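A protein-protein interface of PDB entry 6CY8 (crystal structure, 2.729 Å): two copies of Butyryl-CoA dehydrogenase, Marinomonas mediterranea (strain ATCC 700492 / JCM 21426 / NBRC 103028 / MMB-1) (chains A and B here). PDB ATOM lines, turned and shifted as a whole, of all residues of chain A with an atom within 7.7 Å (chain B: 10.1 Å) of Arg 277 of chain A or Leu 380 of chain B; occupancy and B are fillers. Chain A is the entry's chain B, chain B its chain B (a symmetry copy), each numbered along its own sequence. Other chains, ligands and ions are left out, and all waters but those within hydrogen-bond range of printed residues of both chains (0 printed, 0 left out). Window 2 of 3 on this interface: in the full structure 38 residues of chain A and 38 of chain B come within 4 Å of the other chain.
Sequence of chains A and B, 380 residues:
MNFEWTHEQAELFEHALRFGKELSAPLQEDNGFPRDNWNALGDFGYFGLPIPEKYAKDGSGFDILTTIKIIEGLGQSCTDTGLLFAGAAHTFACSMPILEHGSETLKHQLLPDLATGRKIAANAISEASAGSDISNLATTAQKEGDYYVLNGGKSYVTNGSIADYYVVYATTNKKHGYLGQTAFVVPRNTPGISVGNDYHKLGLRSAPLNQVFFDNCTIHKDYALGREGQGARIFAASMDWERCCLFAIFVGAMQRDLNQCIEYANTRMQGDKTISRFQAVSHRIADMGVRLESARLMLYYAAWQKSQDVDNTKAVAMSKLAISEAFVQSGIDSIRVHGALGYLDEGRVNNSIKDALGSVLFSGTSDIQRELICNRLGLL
O of Ala 265 of chain A sits at hydrogen-bond distance from N of Ser 276 of chain A, 3.1 Å away.
The side-chain amide oxygen (OD1) of Asn 266 of chain A lies within hydrogen-bond range of the side-chain hydroxyl (OG) of Ser 276 of chain A, 3.4 Å away.
The side-chain hydroxyl of Ser 276 of chain A lies within hydrogen-bond range of the side-chain hydroxyl of Thr 274 of chain A (3.2 Å).
O of Phe 278 of chain A lies within hydrogen-bond range of OG of Ser 282 of chain A (3.2 Å).
The backbone carbonyl oxygen of Cys 374 of chain B is in hydrogen-bond range of the backbone NH of Leu 379 of chain B.
Among the printed residues, merely in contact across the chains: Ile 262 of chain A with Leu 377 of chain B (3.9 Å), Ala 265 of chain A with Leu 379 of chain B (3.9 Å), Asn 266 of chain A with Leu 379 of chain B (3.3 Å), Ser 276 of chain A with Leu 379 of chain B (3.8 Å) and Ser 276 of chain A with Leu 380 of chain B (3.0 Å).
Of the printed residues of chain B, Ala 265 of chain A touches Leu 379.
Ser 276 of chain A touches just these residues of chain B: Leu 379 (3.8 Å) and Leu 380 (3.0 Å).
Of the printed residues of chain B, Gln 279 of chain A touches Glu 371.
Of the printed residues of chain A, Glu 371 of chain B touches Gln 279 (3.0 Å).
Printed residues of chain A within 4 Å of Leu 377 of chain B: Ile 262.
Printed residues of chain A within 4 Å of Leu 379 of chain B: Ala 265, Asn 266 and Ser 276.
Of chain A, only Asn 266 (2.8 Å), Ser 276 (3.0 Å) and Arg 277 (3.1 Å) come within 4 Å of Leu 380 of chain B.
The nearest residue of chain B that does not touch Arg 277 of chain A is Glu 371 of chain B (6.7 Å).
O of Gly 378 of chain B sits at hydrogen-bond distance from ND2 of Asn 266 of chain A.
The side-chain amide oxygen of Asn 266 of chain A sits at hydrogen-bond distance from the backbone NH of Leu 380 of chain B (2.8 Å).
NE of Arg 277 of chain A is in hydrogen-bond range of O of Leu 380 of chain B, 3.1 Å away.
The side-chain carboxylate (OE2) of Glu 371 of chain B sits at hydrogen-bond distance from the side-chain amide nitrogen (NE2) of Gln 279 of chain A, at 3.0 Å.
The side-chain sulfur (SG) of Cys 374 of chain B sits at hydrogen-bond distance from the backbone carbonyl oxygen (O) of Ser 282 of chain A (3.1 Å).
Hydrophobic or aromatic side chains of chain A within 4 Å of the printed part of chain B: Ile 262 and Ala 265.
Hydrophobic or aromatic side chains of chain B within 4 Å of the printed part of chain A: Leu 379 and Leu 380.
Along chain B the printed residues that touch a printed residue of chain A span positions 371 to 380.
Among the printed residues, no Asp or Glu carboxylate lies within 4 Å of a Lys or Arg side-chain nitrogen of the other chain.
No position is printed for both chains.
Of the 10 pairs that touch across the chains among the printed residues, none has its exchanged pair printed and touching as well.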
ATOM      1  N   ILE A 262       2.113   0.217  22.701  1.00  0.00           N
ATOM      2  CA  ILE A 262       3.310   0.629  21.975  1.00  0.00           C
ATOM      3  C   ILE A 262       4.496   0.696  22.918  1.00  0.00           C
ATOM      4  O   ILE A 262       5.563   0.137  22.644  1.00  0.00           O
ATOM      5  CB  ILE A 262       3.095   1.971  21.255  1.00  0.00           C
ATOM      6  CG1 ILE A 262       2.153   1.790  20.063  1.00  0.00           C
ATOM      7  CG2 ILE A 262       4.427   2.506  20.795  1.00  0.00           C
ATOM      8  CD1 ILE A 262       1.473   3.064  19.594  1.00  0.00           C
ATOM      9  N   ALA A 265       5.446  -2.911  24.038  1.00  0.00           N
ATOM     10  CA  ALA A 265       6.035  -3.768  23.018  1.00  0.00           C
ATOM     11  C   ALA A 265       7.440  -3.309  22.637  1.00  0.00           C
ATOM     12  O   ALA A 265       8.248  -4.120  22.159  1.00  0.00           O
ATOM     13  CB  ALA A 265       5.134  -3.807  21.784  1.00  0.00           C
ATOM     14  N   ASN A 266       7.743  -2.017  22.821  1.00  0.00           N
ATOM     15  CA  ASN A 266       9.076  -1.492  22.533  1.00  0.00           C
ATOM     16  C   ASN A 266      10.063  -1.694  23.677  1.00  0.00           C
ATOM     17  O   ASN A 266      11.264  -1.533  23.455  1.00  0.00           O
ATOM     18  CB  ASN A 266       9.011   0.001  22.182  1.00  0.00           C
ATOM     19  CG  ASN A 266       8.543   0.245  20.758  1.00  0.00           C
ATOM     20  OD1 ASN A 266       8.473  -0.689  19.953  1.00  0.00           O
ATOM     21  ND2 ASN A 266       8.225   1.491  20.436  1.00  0.00           N
ATOM     22  N   THR A 267       9.588  -2.063  24.865  1.00  0.00           N
ATOM     23  CA  THR A 267      10.408  -2.309  26.042  1.00  0.00           C
ATOM     24  C   THR A 267      10.520  -3.783  26.421  1.00  0.00           C
ATOM     25  O   THR A 267      11.598  -4.237  26.824  1.00  0.00           O
ATOM     26  CB  THR A 267       9.831  -1.527  27.225  1.00  0.00           C
ATOM     27  OG1 THR A 267       9.927  -0.125  26.957  1.00  0.00           O
ATOM     28  CG2 THR A 267      10.572  -1.851  28.517  1.00  0.00           C
ATOM     29  N   ARG A 268       9.437  -4.545  26.317  1.00  0.00           N
ATOM     30  CA  ARG A 268       9.450  -5.926  26.777  1.00  0.00           C
ATOM     31  C   ARG A 268      10.251  -6.784  25.819  1.00  0.00           C
ATOM     32  O   ARG A 268      10.033  -6.749  24.605  1.00  0.00           O
ATOM     33  CB  ARG A 268       8.027  -6.470  26.900  1.00  0.00           C
ATOM     34  CG  ARG A 268       7.967  -7.973  27.125  1.00  0.00           C
ATOM     35  CD  ARG A 268       8.572  -8.359  28.471  1.00  0.00           C
ATOM     36  NE  ARG A 268       8.267  -9.734  28.866  1.00  0.00           N
ATOM     37  CZ  ARG A 268       8.552 -10.246  30.061  1.00  0.00           C
ATOM     38  NH1 ARG A 268       9.150  -9.496  30.977  1.00  0.00           N
ATOM     39  NH2 ARG A 268       8.238 -11.505  30.348  1.00  0.00           N
ATOM     40  N   ASP A 272      16.319 -11.472  23.925  1.00  0.00           N
ATOM     41  CA  ASP A 272      17.092 -10.265  23.605  1.00  0.00           C
ATOM     42  C   ASP A 272      16.673  -9.640  22.280  1.00  0.00           C
ATOM     43  O   ASP A 272      17.503  -9.181  21.480  1.00  0.00           O
ATOM     44  CB  ASP A 272      18.593 -10.527  23.635  1.00  0.00           C
ATOM     45  CG  ASP A 272      19.251  -9.913  24.864  1.00  0.00           C
ATOM     46  OD1 ASP A 272      18.539  -9.741  25.888  1.00  0.00           O
ATOM     47  OD2 ASP A 272      20.447  -9.560  24.788  1.00  0.00           O
ATOM     48  N   LYS A 273      15.365  -9.658  22.058  1.00  0.00           N
ATOM     49  CA  LYS A 273      14.675  -8.920  21.018  1.00  0.00           C
ATOM     50  C   LYS A 273      13.408  -8.371  21.664  1.00  0.00           C
ATOM     51  O   LYS A 273      12.828  -9.018  22.545  1.00  0.00           O
ATOM     52  CB  LYS A 273      14.378  -9.857  19.833  1.00  0.00           C
ATOM     53  CG  LYS A 273      14.018  -9.204  18.518  1.00  0.00           C
ATOM     54  CD  LYS A 273      13.374 -10.237  17.584  1.00  0.00           C
ATOM     55  CE  LYS A 273      12.367 -11.076  18.331  1.00  0.00           C
ATOM     56  NZ  LYS A 273      11.348 -10.231  19.037  1.00  0.00           N
ATOM     57  N   THR A 274      13.003  -7.159  21.287  1.00  0.00           N
ATOM     58  CA  THR A 274      11.732  -6.644  21.797  1.00  0.00           C
ATOM     59  C   THR A 274      10.557  -7.258  21.048  1.00  0.00           C
ATOM     60  O   THR A 274      10.619  -7.507  19.840  1.00  0.00           O
ATOM     61  CB  THR A 274      11.622  -5.121  21.692  1.00  0.00           C
ATOM     62  OG1 THR A 274      11.615  -4.722  20.312  1.00  0.00           O
ATOM     63  CG2 THR A 274      12.731  -4.444  22.451  1.00  0.00           C
ATOM     64  N   ILE A 275       9.460  -7.469  21.782  1.00  0.00           N
ATOM     65  CA  ILE A 275       8.361  -8.267  21.256  1.00  0.00           C
ATOM     66  C   ILE A 275       7.708  -7.593  20.062  1.00  0.00           C
ATOM     67  O   ILE A 275       7.120  -8.278  19.218  1.00  0.00           O
ATOM     68  CB  ILE A 275       7.338  -8.576  22.367  1.00  0.00           C
ATOM     69  CG1 ILE A 275       6.708  -7.282  22.895  1.00  0.00           C
ATOM     70  CG2 ILE A 275       8.003  -9.334  23.515  1.00  0.00           C
ATOM     71  CD1 ILE A 275       5.381  -7.493  23.568  1.00  0.00           C
ATOM     72  N   SER A 276       7.830  -6.270  19.944  1.00  0.00           N
ATOM     73  CA  SER A 276       7.380  -5.582  18.736  1.00  0.00           C
ATOM     74  C   SER A 276       8.059  -6.087  17.465  1.00  0.00           C
ATOM     75  O   SER A 276       7.581  -5.796  16.365  1.00  0.00           O
ATOM     76  CB  SER A 276       7.630  -4.085  18.861  1.00  0.00           C
ATOM     77  OG  SER A 276       9.006  -3.828  18.703  1.00  0.00           O
ATOM     78  N   ARG A 277       9.172  -6.800  17.570  1.00  0.00           N
ATOM     79  CA  ARG A 277       9.776  -7.358  16.369  1.00  0.00           C
ATOM     80  C   ARG A 277       9.030  -8.571  15.844  1.00  0.00           C
ATOM     81  O   ARG A 277       9.314  -9.000  14.715  1.00  0.00           O
ATOM     82  CB  ARG A 277      11.239  -7.740  16.626  1.00  0.00           C
ATOM     83  CG  ARG A 277      12.223  -6.585  16.542  1.00  0.00           C
ATOM     84  CD  ARG A 277      12.436  -6.115  15.113  1.00  0.00           C
ATOM     85  NE  ARG A 277      13.397  -5.016  15.073  1.00  0.00           N
ATOM     86  CZ  ARG A 277      14.720  -5.156  15.183  1.00  0.00           C
ATOM     87  NH1 ARG A 277      15.268  -6.365  15.335  1.00  0.00           N
ATOM     88  NH2 ARG A 277      15.498  -4.077  15.136  1.00  0.00           N
ATOM     89  N   PHE A 278       8.137  -9.158  16.651  1.00  0.00           N
ATOM     90  CA  PHE A 278       7.224 -10.192  16.177  1.00  0.00           C
ATOM     91  C   PHE A 278       6.001  -9.548  15.534  1.00  0.00           C
ATOM     92  O   PHE A 278       5.335  -8.702  16.144  1.00  0.00           O
ATOM     93  CB  PHE A 278       6.768 -11.099  17.320  1.00  0.00           C
ATOM     94  CG  PHE A 278       7.888 -11.714  18.094  1.00  0.00           C
ATOM     95  CD1 PHE A 278       8.747 -12.623  17.497  1.00  0.00           C
ATOM     96  CD2 PHE A 278       8.081 -11.393  19.426  1.00  0.00           C
ATOM     97  CE1 PHE A 278       9.786 -13.191  18.211  1.00  0.00           C
ATOM     98  CE2 PHE A 278       9.116 -11.970  20.146  1.00  0.00           C
ATOM     99  CZ  PHE A 278       9.964 -12.870  19.536  1.00  0.00           C
ATOM    100  N   GLN A 279       5.688  -9.971  14.311  1.00  0.00           N
ATOM    101  CA  GLN A 279       4.520  -9.417  13.644  1.00  0.00           C
ATOM    102  C   GLN A 279       3.208  -9.864  14.284  1.00  0.00           C
ATOM    103  O   GLN A 279       2.209  -9.153  14.147  1.00  0.00           O
ATOM    104  CB  GLN A 279       4.541  -9.770  12.163  1.00  0.00           C
ATOM    105  CG  GLN A 279       5.451  -8.852  11.371  1.00  0.00           C
ATOM    106  CD  GLN A 279       5.629  -9.298   9.955  1.00  0.00           C
ATOM    107  OE1 GLN A 279       5.152 -10.374   9.562  1.00  0.00           O
ATOM    108  NE2 GLN A 279       6.302  -8.466   9.158  1.00  0.00           N
ATOM    109  N   ALA A 280       3.180 -10.987  15.012  1.00  0.00           N
ATOM    110  CA  ALA A 280       1.962 -11.323  15.749  1.00  0.00           C
ATOM    111  C   ALA A 280       1.605 -10.236  16.762  1.00  0.00           C
ATOM    112  O   ALA A 280       0.415  -9.957  16.989  1.00  0.00           O
ATOM    113  CB  ALA A 280       2.102 -12.678  16.446  1.00  0.00           C
ATOM    114  N   VAL A 281       2.622  -9.620  17.385  1.00  0.00           N
ATOM    115  CA  VAL A 281       2.399  -8.506  18.302  1.00  0.00           C
ATOM    116  C   VAL A 281       2.171  -7.218  17.519  1.00  0.00           C
ATOM    117  O   VAL A 281       1.153  -6.538  17.697  1.00  0.00           O
ATOM    118  CB  VAL A 281       3.587  -8.351  19.282  1.00  0.00           C
ATOM    119  CG1 VAL A 281       3.490  -7.038  20.097  1.00  0.00           C
ATOM    120  CG2 VAL A 281       3.702  -9.524  20.185  1.00  0.00           C
ATOM    121  N   SER A 282       3.116  -6.861  16.644  1.00  0.00           N
ATOM    122  CA  SER A 282       3.113  -5.509  16.086  1.00  0.00           C
ATOM    123  C   SER A 282       1.923  -5.300  15.166  1.00  0.00           C
ATOM    124  O   SER A 282       1.305  -4.228  15.186  1.00  0.00           O
ATOM    125  CB  SER A 282       4.413  -5.221  15.333  1.00  0.00           C
ATOM    126  OG  SER A 282       4.634  -6.172  14.296  1.00  0.00           O
ATOM    127  N   GLU B 371       3.170  -3.013   8.229  1.00  0.00           N
ATOM    128  CA  GLU B 371       4.566  -2.704   8.529  1.00  0.00           C
ATOM    129  C   GLU B 371       4.804  -1.198   8.560  1.00  0.00           C
ATOM    130  O   GLU B 371       5.442  -0.680   9.486  1.00  0.00           O
ATOM    131  CB  GLU B 371       5.481  -3.373   7.500  1.00  0.00           C
ATOM    132  CG  GLU B 371       5.682  -4.852   7.737  1.00  0.00           C
ATOM    133  CD  GLU B 371       6.489  -5.130   8.993  1.00  0.00           C
ATOM    134  OE1 GLU B 371       7.710  -4.850   8.999  1.00  0.00           O
ATOM    135  OE2 GLU B 371       5.912  -5.640   9.971  1.00  0.00           O
ATOM    136  N   LEU B 372       4.275  -0.481   7.565  1.00  0.00           N
ATOM    137  CA  LEU B 372       4.347   0.980   7.572  1.00  0.00           C
ATOM    138  C   LEU B 372       3.643   1.559   8.788  1.00  0.00           C
ATOM    139  O   LEU B 372       4.203   2.403   9.497  1.00  0.00           O
ATOM    140  CB  LEU B 372       3.741   1.555   6.287  1.00  0.00           C
ATOM    141  CG  LEU B 372       4.534   1.315   4.998  1.00  0.00           C
ATOM    142  CD1 LEU B 372       3.599   1.130   3.802  1.00  0.00           C
ATOM    143  CD2 LEU B 372       5.546   2.439   4.766  1.00  0.00           C
ATOM    144  N   ILE B 373       2.404   1.121   9.042  1.00  0.00           N
ATOM    145  CA  ILE B 373       1.653   1.632  10.184  1.00  0.00           C
ATOM    146  C   ILE B 373       2.449   1.433  11.473  1.00  0.00           C
ATOM    147  O   ILE B 373       2.676   2.384  12.230  1.00  0.00           O
ATOM    148  CB  ILE B 373       0.258   0.976  10.244  1.00  0.00           C
ATOM    149  CG1 ILE B 373      -0.589   1.472   9.060  1.00  0.00           C
ATOM    150  CG2 ILE B 373      -0.435   1.290  11.572  1.00  0.00           C
ATOM    151  CD1 ILE B 373      -1.766   0.574   8.655  1.00  0.00           C
ATOM    152  N   CYS B 374       2.914   0.203  11.716  1.00  0.00           N
ATOM    153  CA  CYS B 374       3.751  -0.078  12.882  1.00  0.00           C
ATOM    154  C   CYS B 374       4.900   0.911  12.992  1.00  0.00           C
ATOM    155  O   CYS B 374       5.152   1.479  14.064  1.00  0.00           O
ATOM    156  CB  CYS B 374       4.324  -1.494  12.796  1.00  0.00           C
ATOM    157  SG  CYS B 374       3.141  -2.779  13.083  1.00  0.00           S
ATOM    158  N   ASN B 375       5.624   1.095  11.887  1.00  0.00           N
ATOM    159  CA  ASN B 375       6.742   2.020  11.849  1.00  0.00           C
ATOM    160  C   ASN B 375       6.326   3.412  12.319  1.00  0.00           C
ATOM    161  O   ASN B 375       6.892   3.963  13.275  1.00  0.00           O
ATOM    162  CB  ASN B 375       7.295   2.051  10.425  1.00  0.00           C
ATOM    163  CG  ASN B 375       8.506   2.946  10.283  1.00  0.00           C
ATOM    164  OD1 ASN B 375       8.414   4.029   9.711  1.00  0.00           O
ATOM    165  ND2 ASN B 375       9.650   2.498  10.808  1.00  0.00           N
ATOM    166  N   ARG B 376       5.297   3.980  11.682  1.00  0.00           N
ATOM    167  CA  ARG B 376       4.863   5.329  12.021  1.00  0.00           C
ATOM    168  C   ARG B 376       4.268   5.415  13.421  1.00  0.00           C
ATOM    169  O   ARG B 376       4.118   6.521  13.950  1.00  0.00           O
ATOM    170  CB  ARG B 376       3.840   5.832  11.000  1.00  0.00           C
ATOM    171  CG  ARG B 376       4.394   6.052   9.598  1.00  0.00           C
ATOM    172  CD  ARG B 376       5.666   6.902   9.610  1.00  0.00           C
ATOM    173  NE  ARG B 376       6.051   7.379   8.278  1.00  0.00           N
ATOM    174  CZ  ARG B 376       6.669   6.634   7.360  1.00  0.00           C
ATOM    175  NH1 ARG B 376       6.965   5.370   7.621  1.00  0.00           N
ATOM    176  NH2 ARG B 376       6.986   7.151   6.181  1.00  0.00           N
ATOM    177  N   LEU B 377       3.898   4.286  14.021  1.00  0.00           N
ATOM    178  CA  LEU B 377       3.419   4.314  15.394  1.00  0.00           C
ATOM    179  C   LEU B 377       4.559   4.336  16.399  1.00  0.00           C
ATOM    180  O   LEU B 377       4.331   4.675  17.567  1.00  0.00           O
ATOM    181  CB  LEU B 377       2.521   3.109  15.688  1.00  0.00           C
ATOM    182  CG  LEU B 377       1.111   3.046  15.114  1.00  0.00           C
ATOM    183  CD1 LEU B 377       0.502   1.685  15.426  1.00  0.00           C
ATOM    184  CD2 LEU B 377       0.246   4.166  15.657  1.00  0.00           C
ATOM    185  N   GLY B 378       5.769   3.982  15.973  1.00  0.00           N
ATOM    186  CA  GLY B 378       6.920   3.943  16.844  1.00  0.00           C
ATOM    187  C   GLY B 378       7.412   2.556  17.166  1.00  0.00           C
ATOM    188  O   GLY B 378       8.418   2.421  17.879  1.00  0.00           O
ATOM    189  N   LEU B 379       6.748   1.517  16.671  1.00  0.00           N
ATOM    190  CA  LEU B 379       7.151   0.164  17.018  1.00  0.00           C
ATOM    191  C   LEU B 379       8.517  -0.150  16.427  1.00  0.00           C
ATOM    192  O   LEU B 379       8.752   0.025  15.226  1.00  0.00           O
ATOM    193  CB  LEU B 379       6.111  -0.836  16.532  1.00  0.00           C
ATOM    194  CG  LEU B 379       4.804  -0.714  17.305  1.00  0.00           C
ATOM    195  CD1 LEU B 379       3.687  -1.291  16.503  1.00  0.00           C
ATOM    196  CD2 LEU B 379       4.938  -1.423  18.653  1.00  0.00           C
ATOM    197  N   LEU B 380       9.425  -0.589  17.285  1.00  0.00           N
ATOM    198  CA  LEU B 380      10.702  -1.098  16.830  1.00  0.00           C
ATOM    199  C   LEU B 380      10.517  -2.545  16.401  1.00  0.00           C
ATOM    200  O   LEU B 380      11.076  -2.977  15.393  1.00  0.00           O
ATOM    201  CB  LEU B 380      11.768  -0.971  17.925  1.00  0.00           C
ATOM    202  CG  LEU B 380      11.765   0.362  18.688  1.00  0.00           C
ATOM    203  CD1 LEU B 380      12.591   0.246  19.964  1.00  0.00           C
ATOM    204  CD2 LEU B 380      12.254   1.523  17.818  1.00  0.00           C
